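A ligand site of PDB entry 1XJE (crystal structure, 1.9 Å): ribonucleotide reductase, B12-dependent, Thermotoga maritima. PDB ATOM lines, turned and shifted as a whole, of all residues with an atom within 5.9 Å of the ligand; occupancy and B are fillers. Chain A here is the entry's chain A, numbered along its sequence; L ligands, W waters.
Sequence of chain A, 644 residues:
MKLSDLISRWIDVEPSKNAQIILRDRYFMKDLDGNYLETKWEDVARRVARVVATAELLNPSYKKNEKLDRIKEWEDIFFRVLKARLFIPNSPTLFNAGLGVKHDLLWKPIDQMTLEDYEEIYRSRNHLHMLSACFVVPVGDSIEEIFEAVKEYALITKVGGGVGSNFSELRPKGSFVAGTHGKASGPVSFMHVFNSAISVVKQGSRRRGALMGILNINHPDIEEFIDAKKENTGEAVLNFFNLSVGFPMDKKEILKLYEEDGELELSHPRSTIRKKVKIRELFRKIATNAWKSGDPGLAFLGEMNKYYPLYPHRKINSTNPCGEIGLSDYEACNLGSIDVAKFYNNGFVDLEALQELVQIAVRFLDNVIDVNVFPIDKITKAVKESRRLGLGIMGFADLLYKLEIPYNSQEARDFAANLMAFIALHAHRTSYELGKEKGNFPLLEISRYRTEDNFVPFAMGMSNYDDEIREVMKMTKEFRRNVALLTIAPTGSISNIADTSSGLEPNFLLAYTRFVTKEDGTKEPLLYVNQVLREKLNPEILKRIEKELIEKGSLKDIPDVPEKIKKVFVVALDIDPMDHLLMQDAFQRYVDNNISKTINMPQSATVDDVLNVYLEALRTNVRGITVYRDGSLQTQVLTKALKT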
ATOM      1  N   TYR A  27     -18.131  -0.054  -6.729  1.00  0.00           N
ATOM      2  CA  TYR A  27     -19.522  -0.475  -6.380  1.00  0.00           C
ATOM      3  C   TYR A  27     -20.551   0.663  -6.388  1.00  0.00           C
ATOM      4  O   TYR A  27     -21.736   0.463  -6.687  1.00  0.00           O
ATOM      5  CB  TYR A  27     -19.560  -1.311  -5.084  1.00  0.00           C
ATOM      6  CG  TYR A  27     -18.902  -2.686  -5.243  1.00  0.00           C
ATOM      7  CD1 TYR A  27     -17.515  -2.856  -5.068  1.00  0.00           C
ATOM      8  CD2 TYR A  27     -19.652  -3.811  -5.606  1.00  0.00           C
ATOM      9  CE1 TYR A  27     -16.909  -4.098  -5.209  1.00  0.00           C
ATOM     10  CE2 TYR A  27     -19.073  -5.044  -5.756  1.00  0.00           C
ATOM     11  CZ  TYR A  27     -17.684  -5.189  -5.562  1.00  0.00           C
ATOM     12  OH  TYR A  27     -17.101  -6.400  -5.772  1.00  0.00           O
ATOM     13  N   PRO A  89     -24.909 -10.595  -1.839  1.00  0.00           N
ATOM     14  CA  PRO A  89     -24.922 -11.307  -3.125  1.00  0.00           C
ATOM     15  C   PRO A  89     -23.606 -11.101  -3.900  1.00  0.00           C
ATOM     16  O   PRO A  89     -22.869 -10.138  -3.648  1.00  0.00           O
ATOM     17  CB  PRO A  89     -26.055 -10.672  -3.898  1.00  0.00           C
ATOM     18  CG  PRO A  89     -26.079  -9.264  -3.337  1.00  0.00           C
ATOM     19  CD  PRO A  89     -25.668  -9.333  -1.906  1.00  0.00           C
ATOM     20  N   ASN A  90     -23.350 -11.991  -4.849  1.00  0.00           N
ATOM     21  CA  ASN A  90     -22.200 -11.857  -5.753  1.00  0.00           C
ATOM     22  C   ASN A  90     -22.092 -10.493  -6.416  1.00  0.00           C
ATOM     23  O   ASN A  90     -23.083  -9.821  -6.673  1.00  0.00           O
ATOM     24  CB  ASN A  90     -22.081 -13.027  -6.755  1.00  0.00           C
ATOM     25  CG  ASN A  90     -23.255 -13.198  -7.732  1.00  0.00           C
ATOM     26  OD1 ASN A  90     -23.361 -14.253  -8.358  1.00  0.00           O
ATOM     27  ND2 ASN A  90     -24.133 -12.180  -7.869  1.00  0.00           N
ATOM     28  N   SER A  91     -20.849 -10.082  -6.697  1.00  0.00           N
ATOM     29  CA  SER A  91     -20.603  -8.715  -7.151  1.00  0.00           C
ATOM     30  C   SER A  91     -21.527  -8.215  -8.269  1.00  0.00           C
ATOM     31  O   SER A  91     -21.958  -7.080  -8.219  1.00  0.00           O
ATOM     32  CB  SER A  91     -19.127  -8.524  -7.509  1.00  0.00           C
ATOM     33  OG  SER A  91     -18.358  -8.566  -6.321  1.00  0.00           O
ATOM     34  N   PRO A  92     -21.791  -9.023  -9.298  1.00  0.00           N
ATOM     35  CA  PRO A  92     -22.596  -8.483 -10.408  1.00  0.00           C
ATOM     36  C   PRO A  92     -24.014  -8.034 -10.047  1.00  0.00           C
ATOM     37  O   PRO A  92     -24.517  -7.119 -10.662  1.00  0.00           O
ATOM     38  CB  PRO A  92     -22.652  -9.628 -11.390  1.00  0.00           C
ATOM     39  CG  PRO A  92     -21.432 -10.478 -11.063  1.00  0.00           C
ATOM     40  CD  PRO A  92     -21.351 -10.385  -9.583  1.00  0.00           C
ATOM     41  N   ALA A 133     -22.881 -14.379 -11.528  1.00  0.00           N
ATOM     42  CA  ALA A 133     -21.401 -14.450 -11.657  1.00  0.00           C
ATOM     43  C   ALA A 133     -20.835 -15.594 -12.489  1.00  0.00           C
ATOM     44  O   ALA A 133     -19.644 -15.544 -12.822  1.00  0.00           O
ATOM     45  CB  ALA A 133     -20.800 -14.526 -10.270  1.00  0.00           C
ATOM     46  N   CYS A 134     -21.617 -16.659 -12.735  1.00  0.00           N
ATOM     47  CA  CYS A 134     -21.117 -17.963 -13.203  1.00  0.00           C
ATOM     48  C   CYS A 134     -21.839 -18.454 -14.440  1.00  0.00           C
ATOM     49  O   CYS A 134     -23.077 -18.547 -14.424  1.00  0.00           O
ATOM     50  CB  CYS A 134     -21.288 -19.030 -12.149  1.00  0.00           C
ATOM     51  SG  CYS A 134     -20.615 -18.573 -10.513  1.00  0.00           S
ATOM     52  N   PHE A 135     -21.078 -18.750 -15.508  1.00  0.00           N
ATOM     53  CA  PHE A 135     -21.654 -19.192 -16.802  1.00  0.00           C
ATOM     54  C   PHE A 135     -20.883 -20.370 -17.362  1.00  0.00           C
ATOM     55  O   PHE A 135     -19.673 -20.501 -17.117  1.00  0.00           O
ATOM     56  CB  PHE A 135     -21.581 -18.086 -17.854  1.00  0.00           C
ATOM     57  CG  PHE A 135     -22.483 -16.920 -17.628  1.00  0.00           C
ATOM     58  CD1 PHE A 135     -22.186 -15.949 -16.705  1.00  0.00           C
ATOM     59  CD2 PHE A 135     -23.646 -16.775 -18.414  1.00  0.00           C
ATOM     60  CE1 PHE A 135     -22.999 -14.867 -16.556  1.00  0.00           C
ATOM     61  CE2 PHE A 135     -24.474 -15.720 -18.246  1.00  0.00           C
ATOM     62  CZ  PHE A 135     -24.158 -14.754 -17.316  1.00  0.00           C
ATOM     63  N   THR A 157     -18.555 -11.472 -20.785  1.00  0.00           N
ATOM     64  CA  THR A 157     -17.531 -10.652 -20.154  1.00  0.00           C
ATOM     65  C   THR A 157     -17.848  -9.167 -20.050  1.00  0.00           C
ATOM     66  O   THR A 157     -17.461  -8.533 -19.054  1.00  0.00           O
ATOM     67  CB  THR A 157     -16.208 -10.814 -20.935  1.00  0.00           C
ATOM     68  OG1 THR A 157     -15.948 -12.213 -20.925  1.00  0.00           O
ATOM     69  CG2 THR A 157     -15.054 -10.055 -20.323  1.00  0.00           C
ATOM     70  N   GLY A 160     -19.950  -8.608 -17.034  1.00  0.00           N
ATOM     71  CA  GLY A 160     -19.237  -8.925 -15.840  1.00  0.00           C
ATOM     72  C   GLY A 160     -19.385 -10.365 -15.353  1.00  0.00           C
ATOM     73  O   GLY A 160     -19.093 -10.630 -14.205  1.00  0.00           O
ATOM     74  N   GLY A 161     -19.835 -11.283 -16.202  1.00  0.00           N
ATOM     75  CA  GLY A 161     -19.836 -12.671 -15.839  1.00  0.00           C
ATOM     76  C   GLY A 161     -18.540 -13.423 -16.061  1.00  0.00           C
ATOM     77  O   GLY A 161     -17.729 -13.051 -16.884  1.00  0.00           O
ATOM     78  N   GLY A 162     -18.339 -14.477 -15.304  1.00  0.00           N
ATOM     79  CA  GLY A 162     -17.235 -15.428 -15.535  1.00  0.00           C
ATOM     80  C   GLY A 162     -17.722 -16.696 -16.245  1.00  0.00           C
ATOM     81  O   GLY A 162     -18.676 -17.317 -15.810  1.00  0.00           O
ATOM     82  N   VAL A 163     -17.009 -17.139 -17.277  1.00  0.00           N
ATOM     83  CA  VAL A 163     -17.485 -18.197 -18.146  1.00  0.00           C
ATOM     84  C   VAL A 163     -16.459 -19.297 -18.320  1.00  0.00           C
ATOM     85  O   VAL A 163     -15.272 -19.059 -18.405  1.00  0.00           O
ATOM     86  CB  VAL A 163     -17.881 -17.638 -19.557  1.00  0.00           C
ATOM     87  CG1 VAL A 163     -16.782 -16.888 -20.230  1.00  0.00           C
ATOM     88  CG2 VAL A 163     -18.435 -18.718 -20.444  1.00  0.00           C
ATOM     89  N   ARG A 207     -14.074  -4.807 -13.526  1.00  0.00           N
ATOM     90  CA  ARG A 207     -13.963  -6.270 -13.589  1.00  0.00           C
ATOM     91  C   ARG A 207     -13.371  -6.826 -14.947  1.00  0.00           C
ATOM     92  O   ARG A 207     -14.021  -6.717 -15.971  1.00  0.00           O
ATOM     93  CB  ARG A 207     -15.376  -6.794 -13.270  1.00  0.00           C
ATOM     94  CG  ARG A 207     -15.628  -8.234 -13.475  1.00  0.00           C
ATOM     95  CD  ARG A 207     -16.746  -8.779 -12.590  1.00  0.00           C
ATOM     96  NE  ARG A 207     -16.293  -8.871 -11.205  1.00  0.00           N
ATOM     97  CZ  ARG A 207     -16.656  -9.817 -10.347  1.00  0.00           C
ATOM     98  NH1 ARG A 207     -17.483 -10.790 -10.698  1.00  0.00           N
ATOM     99  NH2 ARG A 207     -16.142  -9.792  -9.126  1.00  0.00           N
ATOM    100  N   ARG A 208     -12.162  -7.423 -14.934  1.00  0.00           N
ATOM    101  CA  ARG A 208     -11.564  -8.030 -16.134  1.00  0.00           C
ATOM    102  C   ARG A 208     -12.234  -9.390 -16.431  1.00  0.00           C
ATOM    103  O   ARG A 208     -12.944  -9.925 -15.601  1.00  0.00           O
ATOM    104  CB  ARG A 208     -10.046  -8.211 -15.996  1.00  0.00           C
ATOM    105  CG  ARG A 208      -9.597  -9.478 -15.228  1.00  0.00           C
ATOM    106  CD  ARG A 208      -8.283  -9.299 -14.425  1.00  0.00           C
ATOM    107  NE  ARG A 208      -7.381 -10.459 -14.581  1.00  0.00           N
ATOM    108  CZ  ARG A 208      -6.296 -10.501 -15.363  1.00  0.00           C
ATOM    109  NH1 ARG A 208      -5.915  -9.450 -16.080  1.00  0.00           N
ATOM    110  NH2 ARG A 208      -5.578 -11.619 -15.428  1.00  0.00           N
ATOM    111  N   GLY A 209     -11.955  -9.961 -17.602  1.00  0.00           N
ATOM    112  CA  GLY A 209     -12.403 -11.326 -17.906  1.00  0.00           C
ATOM    113  C   GLY A 209     -11.904 -12.436 -16.977  1.00  0.00           C
ATOM    114  O   GLY A 209     -10.766 -12.412 -16.480  1.00  0.00           O
ATOM    115  N   ALA A 210     -12.733 -13.453 -16.787  1.00  0.00           N
ATOM    116  CA  ALA A 210     -12.321 -14.588 -15.950  1.00  0.00           C
ATOM    117  C   ALA A 210     -12.856 -15.820 -16.648  1.00  0.00           C
ATOM    118  O   ALA A 210     -14.074 -15.919 -16.795  1.00  0.00           O
ATOM    119  CB  ALA A 210     -12.932 -14.483 -14.567  1.00  0.00           C
ATOM    120  N   ASN A 320     -17.610 -22.940 -14.007  1.00  0.00           N
ATOM    121  CA  ASN A 320     -17.230 -21.543 -14.178  1.00  0.00           C
ATOM    122  C   ASN A 320     -15.747 -21.390 -13.729  1.00  0.00           C
ATOM    123  O   ASN A 320     -15.165 -22.359 -13.265  1.00  0.00           O
ATOM    124  CB  ASN A 320     -18.142 -20.710 -13.332  1.00  0.00           C
ATOM    125  CG  ASN A 320     -17.903 -20.952 -11.849  1.00  0.00           C
ATOM    126  OD1 ASN A 320     -18.041 -22.071 -11.385  1.00  0.00           O
ATOM    127  ND2 ASN A 320     -17.560 -19.897 -11.108  1.00  0.00           N
ATOM    128  N   PRO A 321     -15.145 -20.190 -13.861  1.00  0.00           N
ATOM    129  CA  PRO A 321     -13.748 -19.939 -13.487  1.00  0.00           C
ATOM    130  C   PRO A 321     -13.175 -20.452 -12.165  1.00  0.00           C
ATOM    131  O   PRO A 321     -12.068 -20.978 -12.176  1.00  0.00           O
ATOM    132  CB  PRO A 321     -13.619 -18.414 -13.617  1.00  0.00           C
ATOM    133  CG  PRO A 321     -14.497 -18.119 -14.674  1.00  0.00           C
ATOM    134  CD  PRO A 321     -15.689 -19.041 -14.559  1.00  0.00           C
ATOM    135  N   CYS A 322     -13.853 -20.322 -11.042  1.00  0.00           N
ATOM    136  CA  CYS A 322     -13.230 -20.754  -9.787  1.00  0.00           C
ATOM    137  C   CYS A 322     -13.616 -22.172  -9.330  1.00  0.00           C
ATOM    138  O   CYS A 322     -13.254 -22.584  -8.229  1.00  0.00           O
ATOM    139  CB  CYS A 322     -13.505 -19.714  -8.710  1.00  0.00           C
ATOM    140  SG  CYS A 322     -12.584 -18.179  -9.077  1.00  0.00           S
ATOM    141  N   GLY A 323     -14.290 -22.920 -10.204  1.00  0.00           N
ATOM    142  CA  GLY A 323     -14.604 -24.320  -9.970  1.00  0.00           C
ATOM    143  C   GLY A 323     -15.897 -24.596  -9.195  1.00  0.00           C
ATOM    144  O   GLY A 323     -16.351 -25.747  -9.062  1.00  0.00           O
ATOM    145  N   GLU A 324     -16.483 -23.563  -8.632  1.00  0.00           N
ATOM    146  CA  GLU A 324     -17.495 -23.808  -7.587  1.00  0.00           C
ATOM    147  C   GLU A 324     -18.882 -24.223  -8.108  1.00  0.00           C
ATOM    148  O   GLU A 324     -19.648 -24.773  -7.353  1.00  0.00           O
ATOM    149  CB  GLU A 324     -17.564 -22.656  -6.590  1.00  0.00           C
ATOM    150  CG  GLU A 324     -18.176 -21.361  -6.957  1.00  0.00           C
ATOM    151  CD  GLU A 324     -17.313 -20.388  -7.700  1.00  0.00           C
ATOM    152  OE1 GLU A 324     -16.341 -20.742  -8.377  1.00  0.00           O
ATOM    153  OE2 GLU A 324     -17.595 -19.211  -7.629  1.00  0.00           O
ATOM    154  N   LEU A 335     -24.981 -16.194  -7.106  1.00  0.00           N
ATOM    155  CA  LEU A 335     -24.469 -16.561  -5.824  1.00  0.00           C
ATOM    156  C   LEU A 335     -24.714 -15.486  -4.769  1.00  0.00           C
ATOM    157  O   LEU A 335     -24.969 -14.320  -5.108  1.00  0.00           O
ATOM    158  CB  LEU A 335     -22.926 -16.752  -5.927  1.00  0.00           C
ATOM    159  CG  LEU A 335     -22.230 -17.516  -7.075  1.00  0.00           C
ATOM    160  CD1 LEU A 335     -20.686 -17.534  -6.864  1.00  0.00           C
ATOM    161  CD2 LEU A 335     -22.700 -18.893  -7.198  1.00  0.00           C
ATOM    162  N   ALA A 489     -18.083 -20.070  -2.367  1.00  0.00           N
ATOM    163  CA  ALA A 489     -17.336 -19.325  -3.366  1.00  0.00           C
ATOM    164  C   ALA A 489     -16.063 -18.767  -2.739  1.00  0.00           C
ATOM    165  O   ALA A 489     -15.893 -18.795  -1.528  1.00  0.00           O
ATOM    166  CB  ALA A 489     -18.207 -18.199  -3.875  1.00  0.00           C
ATOM    167  N   PRO A 490     -15.204 -18.192  -3.548  1.00  0.00           N
ATOM    168  CA  PRO A 490     -14.016 -17.508  -3.068  1.00  0.00           C
ATOM    169  C   PRO A 490     -14.311 -16.275  -2.203  1.00  0.00           C
ATOM    170  O   PRO A 490     -13.608 -16.020  -1.192  1.00  0.00           O
ATOM    171  CB  PRO A 490     -13.309 -17.151  -4.372  1.00  0.00           C
ATOM    172  CG  PRO A 490     -13.801 -18.065  -5.351  1.00  0.00           C
ATOM    173  CD  PRO A 490     -15.230 -18.251  -5.028  1.00  0.00           C
ATOM    174  N   THR A 491     -15.356 -15.541  -2.567  1.00  0.00           N
ATOM    175  CA  THR A 491     -15.722 -14.278  -1.916  1.00  0.00           C
ATOM    176  C   THR A 491     -14.579 -13.233  -1.903  1.00  0.00           C
ATOM    177  O   THR A 491     -14.431 -12.419  -0.980  1.00  0.00           O
ATOM    178  CB  THR A 491     -16.374 -14.472  -0.527  1.00  0.00           C
ATOM    179  OG1 THR A 491     -15.387 -14.953   0.397  1.00  0.00           O
ATOM    180  CG2 THR A 491     -17.562 -15.442  -0.629  1.00  0.00           C
ATOM    181  N   GLY A 492     -13.821 -13.207  -2.989  1.00  0.00           N
ATOM    182  CA  GLY A 492     -12.662 -12.374  -3.055  1.00  0.00           C
ATOM    183  C   GLY A 492     -12.963 -10.898  -2.879  1.00  0.00           C
ATOM    184  O   GLY A 492     -12.146 -10.194  -2.329  1.00  0.00           O
ATOM    185  N   SER A 493     -14.137 -10.431  -3.335  1.00  0.00           N
ATOM    186  CA  SER A 493     -14.535  -9.049  -3.093  1.00  0.00           C
ATOM    187  C   SER A 493     -15.567  -8.869  -1.987  1.00  0.00           C
ATOM    188  O   SER A 493     -15.441  -7.966  -1.171  1.00  0.00           O
ATOM    189  CB  SER A 493     -15.058  -8.456  -4.392  1.00  0.00           C
ATOM    190  OG  SER A 493     -14.024  -8.375  -5.329  1.00  0.00           O
ATOM    191  N   ILE A 494     -16.540  -9.773  -1.883  1.00  0.00           N
ATOM    192  CA  ILE A 494     -17.604  -9.525  -0.939  1.00  0.00           C
ATOM    193  C   ILE A 494     -17.151  -9.751   0.484  1.00  0.00           C
ATOM    194  O   ILE A 494     -17.716  -9.114   1.391  1.00  0.00           O
ATOM    195  CB  ILE A 494     -18.976 -10.201  -1.294  1.00  0.00           C
ATOM    196  CG1 ILE A 494     -18.877 -11.713  -1.366  1.00  0.00           C
ATOM    197  CG2 ILE A 494     -19.512  -9.657  -2.602  1.00  0.00           C
ATOM    198  CD1 ILE A 494     -20.221 -12.431  -1.426  1.00  0.00           C
ATOM    199  N   SER A 495     -16.113 -10.566   0.696  1.00  0.00           N
ATOM    200  CA  SER A 495     -15.579 -10.740   2.058  1.00  0.00           C
ATOM    201  C   SER A 495     -14.821  -9.497   2.506  1.00  0.00           C
ATOM    202  O   SER A 495     -14.828  -9.167   3.691  1.00  0.00           O
ATOM    203  CB  SER A 495     -14.751 -12.028   2.159  1.00  0.00           C
ATOM    204  OG  SER A 495     -13.545 -11.916   1.455  1.00  0.00           O
HETATM  205  P1  LIG L   1     -17.306 -11.726  -5.609  1.00  0.00           P
HETATM  206  O1  LIG L   1     -16.838 -10.602  -6.446  1.00  0.00           O
HETATM  207  O2  LIG L   1     -18.797 -11.892  -5.567  1.00  0.00           O
HETATM  208  O3  LIG L   1     -16.653 -11.687  -4.266  1.00  0.00           O
HETATM  209  O4  LIG L   1     -16.810 -13.057  -6.346  1.00  0.00           O
HETATM  210  P2  LIG L   1     -16.161 -14.440  -5.911  1.00  0.00           P
HETATM  211  O5  LIG L   1     -16.926 -15.214  -4.883  1.00  0.00           O
HETATM  212  O6  LIG L   1     -14.719 -14.255  -5.696  1.00  0.00           O
HETATM  213  O7  LIG L   1     -16.144 -15.296  -7.317  1.00  0.00           O
HETATM  214  C1  LIG L   1     -17.280 -16.057  -7.764  1.00  0.00           C
HETATM  215  C2  LIG L   1     -17.431 -16.016  -9.303  1.00  0.00           C
HETATM  216  O8  LIG L   1     -17.351 -14.643  -9.749  1.00  0.00           O
HETATM  217  C3  LIG L   1     -16.175 -16.640  -9.867  1.00  0.00           C
HETATM  218  O9  LIG L   1     -16.205 -18.025  -9.640  1.00  0.00           O
HETATM  219  C4  LIG L   1     -16.259 -16.155 -11.322  1.00  0.00           C
HETATM  220  O10 LIG L   1     -17.166 -17.015 -12.072  1.00  0.00           O
HETATM  221  C5  LIG L   1     -16.762 -14.704 -11.095  1.00  0.00           C
HETATM  222  N1  LIG L   1     -15.638 -13.733 -10.965  1.00  0.00           N
HETATM  223  C6  LIG L   1     -14.892 -13.513  -9.856  1.00  0.00           C
HETATM  224  N2  LIG L   1     -13.976 -12.572 -10.143  1.00  0.00           N
HETATM  225  C7  LIG L   1     -14.152 -12.198 -11.434  1.00  0.00           C
HETATM  226  C8  LIG L   1     -13.512 -11.291 -12.296  1.00  0.00           C
HETATM  227  O11 LIG L   1     -12.564 -10.541 -11.958  1.00  0.00           O
HETATM  228  N3  LIG L   1     -14.010 -11.187 -13.606  1.00  0.00           N
HETATM  229  C9  LIG L   1     -15.101 -11.888 -14.060  1.00  0.00           C
HETATM  230  N4  LIG L   1     -15.499 -11.708 -15.304  1.00  0.00           N
HETATM  231  N5  LIG L   1     -15.671 -12.784 -13.232  1.00  0.00           N
HETATM  232  C10 LIG L   1     -15.225 -12.943 -11.951  1.00  0.00           C
HETATM  233  O   HOH W   1     -15.840  -9.058 -16.843  1.00  0.00           O
HETATM  234  O   HOH W   2     -19.491 -14.252  -4.601  1.00  0.00           O
HETATM  235  O   HOH W   3     -18.733 -12.354  -8.479  1.00  0.00           O
HETATM  236  O   HOH W   4     -12.567 -14.957  -6.943  1.00  0.00           O
HETATM  237  O   HOH W   5     -15.275 -13.347 -18.284  1.00  0.00           O
HETATM  238  O   HOH W   6     -12.591 -15.523 -11.103  1.00  0.00           O
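O9 of the ligand lies within hydrogen-bond range of OE2 of Glu 324. The backbone NH of Ser 493 is in hydrogen-bond range of an oxygen (O3) of the ligand (3.0 Å). The backbone NH (N) of Thr 491 sits at hydrogen-bond distance from an oxygen (O5) of the ligand (2.8 Å). O of Gly 161 is in hydrogen-bond range of N4 of the ligand (3.0 Å). O1 of the ligand is in salt-bridge range of NH2 of Arg 207, at 2.9 Å. SG of Cys 322 lies close to O9 of the ligand, 3.7 Å away. ND2 of Asn 320 sits at hydrogen-bond distance from O9 of the ligand. An oxygen (O3) of the ligand sits at hydrogen-bond distance from the backbone NH of Ile 494, 3.1 Å away. The backbone NH (N) of Gly 492 sits at hydrogen-bond distance from an oxygen (O6) of the ligand (3.0 Å). The backbone carbonyl oxygen of Ala 133 sits at hydrogen-bond distance from an oxygen (O10) of the ligand (3.0 Å). The backbone carbonyl oxygen (O) of Arg 208 sits at hydrogen-bond distance from a nitrogen (N3) of the ligand. N of Ser 91 sits at hydrogen-bond distance from O2 of the ligand (3.0 Å). An oxygen (O1) of the ligand sits at hydrogen-bond distance from the side-chain hydroxyl of Ser 91 (2.5 Å).
The side-chain carboxylate (OE1) of Glu 324 sits at hydrogen-bond distance from the side-chain amide nitrogen (ND2) of Asn 320 (3.1 Å). The backbone NH (N) of Leu 335 is in hydrogen-bond range of the side-chain amide oxygen (OD1) of Asn 90, at 2.8 Å. The backbone NH of Ala 133 sits close to the side-chain amide oxygen of Asn 90, 3.2 Å away. OH of Tyr 27 is in hydrogen-bond range of OG of Ser 91, at 2.6 Å. The backbone carbonyl oxygen of Gly 162 sits at hydrogen-bond distance from the backbone NH of Phe 135, at 2.8 Å. O of Thr 491 is in hydrogen-bond range of OG of Ser 495, 2.6 Å away. N of Gly 162 is in hydrogen-bond range of O of Ala 133, 3.0 Å away. The backbone carbonyl oxygen of Ala 210 lies within hydrogen-bond range of the backbone NH of Val 163, at 3.2 Å.
Residues that only touch the ligand: Asn 90 (3.4 Å), Gly 160 (3.9 Å), Gly 162 (3.8 Å), Ala 210 (3.4 Å), Pro 321 (3.5 Å), Leu 335 (3.8 Å), Ala 489 (3.4 Å) and Pro 490 (3.5 Å). Hydrophobic or aromatic side chains within 4 Å of the ligand: Ala 133, Ala 210, Pro 321, Leu 335, Ala 489, Pro 490 and Ile 494. Of the 30 residues printed, 20 come within 4 Å of the ligand. Along chain A the residues within 4 Å of the ligand span positions 90 to 494. The nearest printed residue that does not touch the ligand is Gly 209 (4.03 Å).
Water W3 lies within hydrogen-bond range of an oxygen (O2) of the ligand (2.9 Å) and the guanidinium group (NH1) of Arg 207 (3.0 Å). Water W6 lies within hydrogen-bond range of the side-chain sulfur of Cys 322 and a nitrogen (N2) of the ligand. Water W5 lies within hydrogen-bond range of the backbone carbonyl oxygen of Gly 161 (2.8 Å), the backbone NH of Ala 210 (3.0 Å), the side-chain hydroxyl of Thr 157 (3.0 Å) and a nitrogen (N4) of the ligand (3.4 Å).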
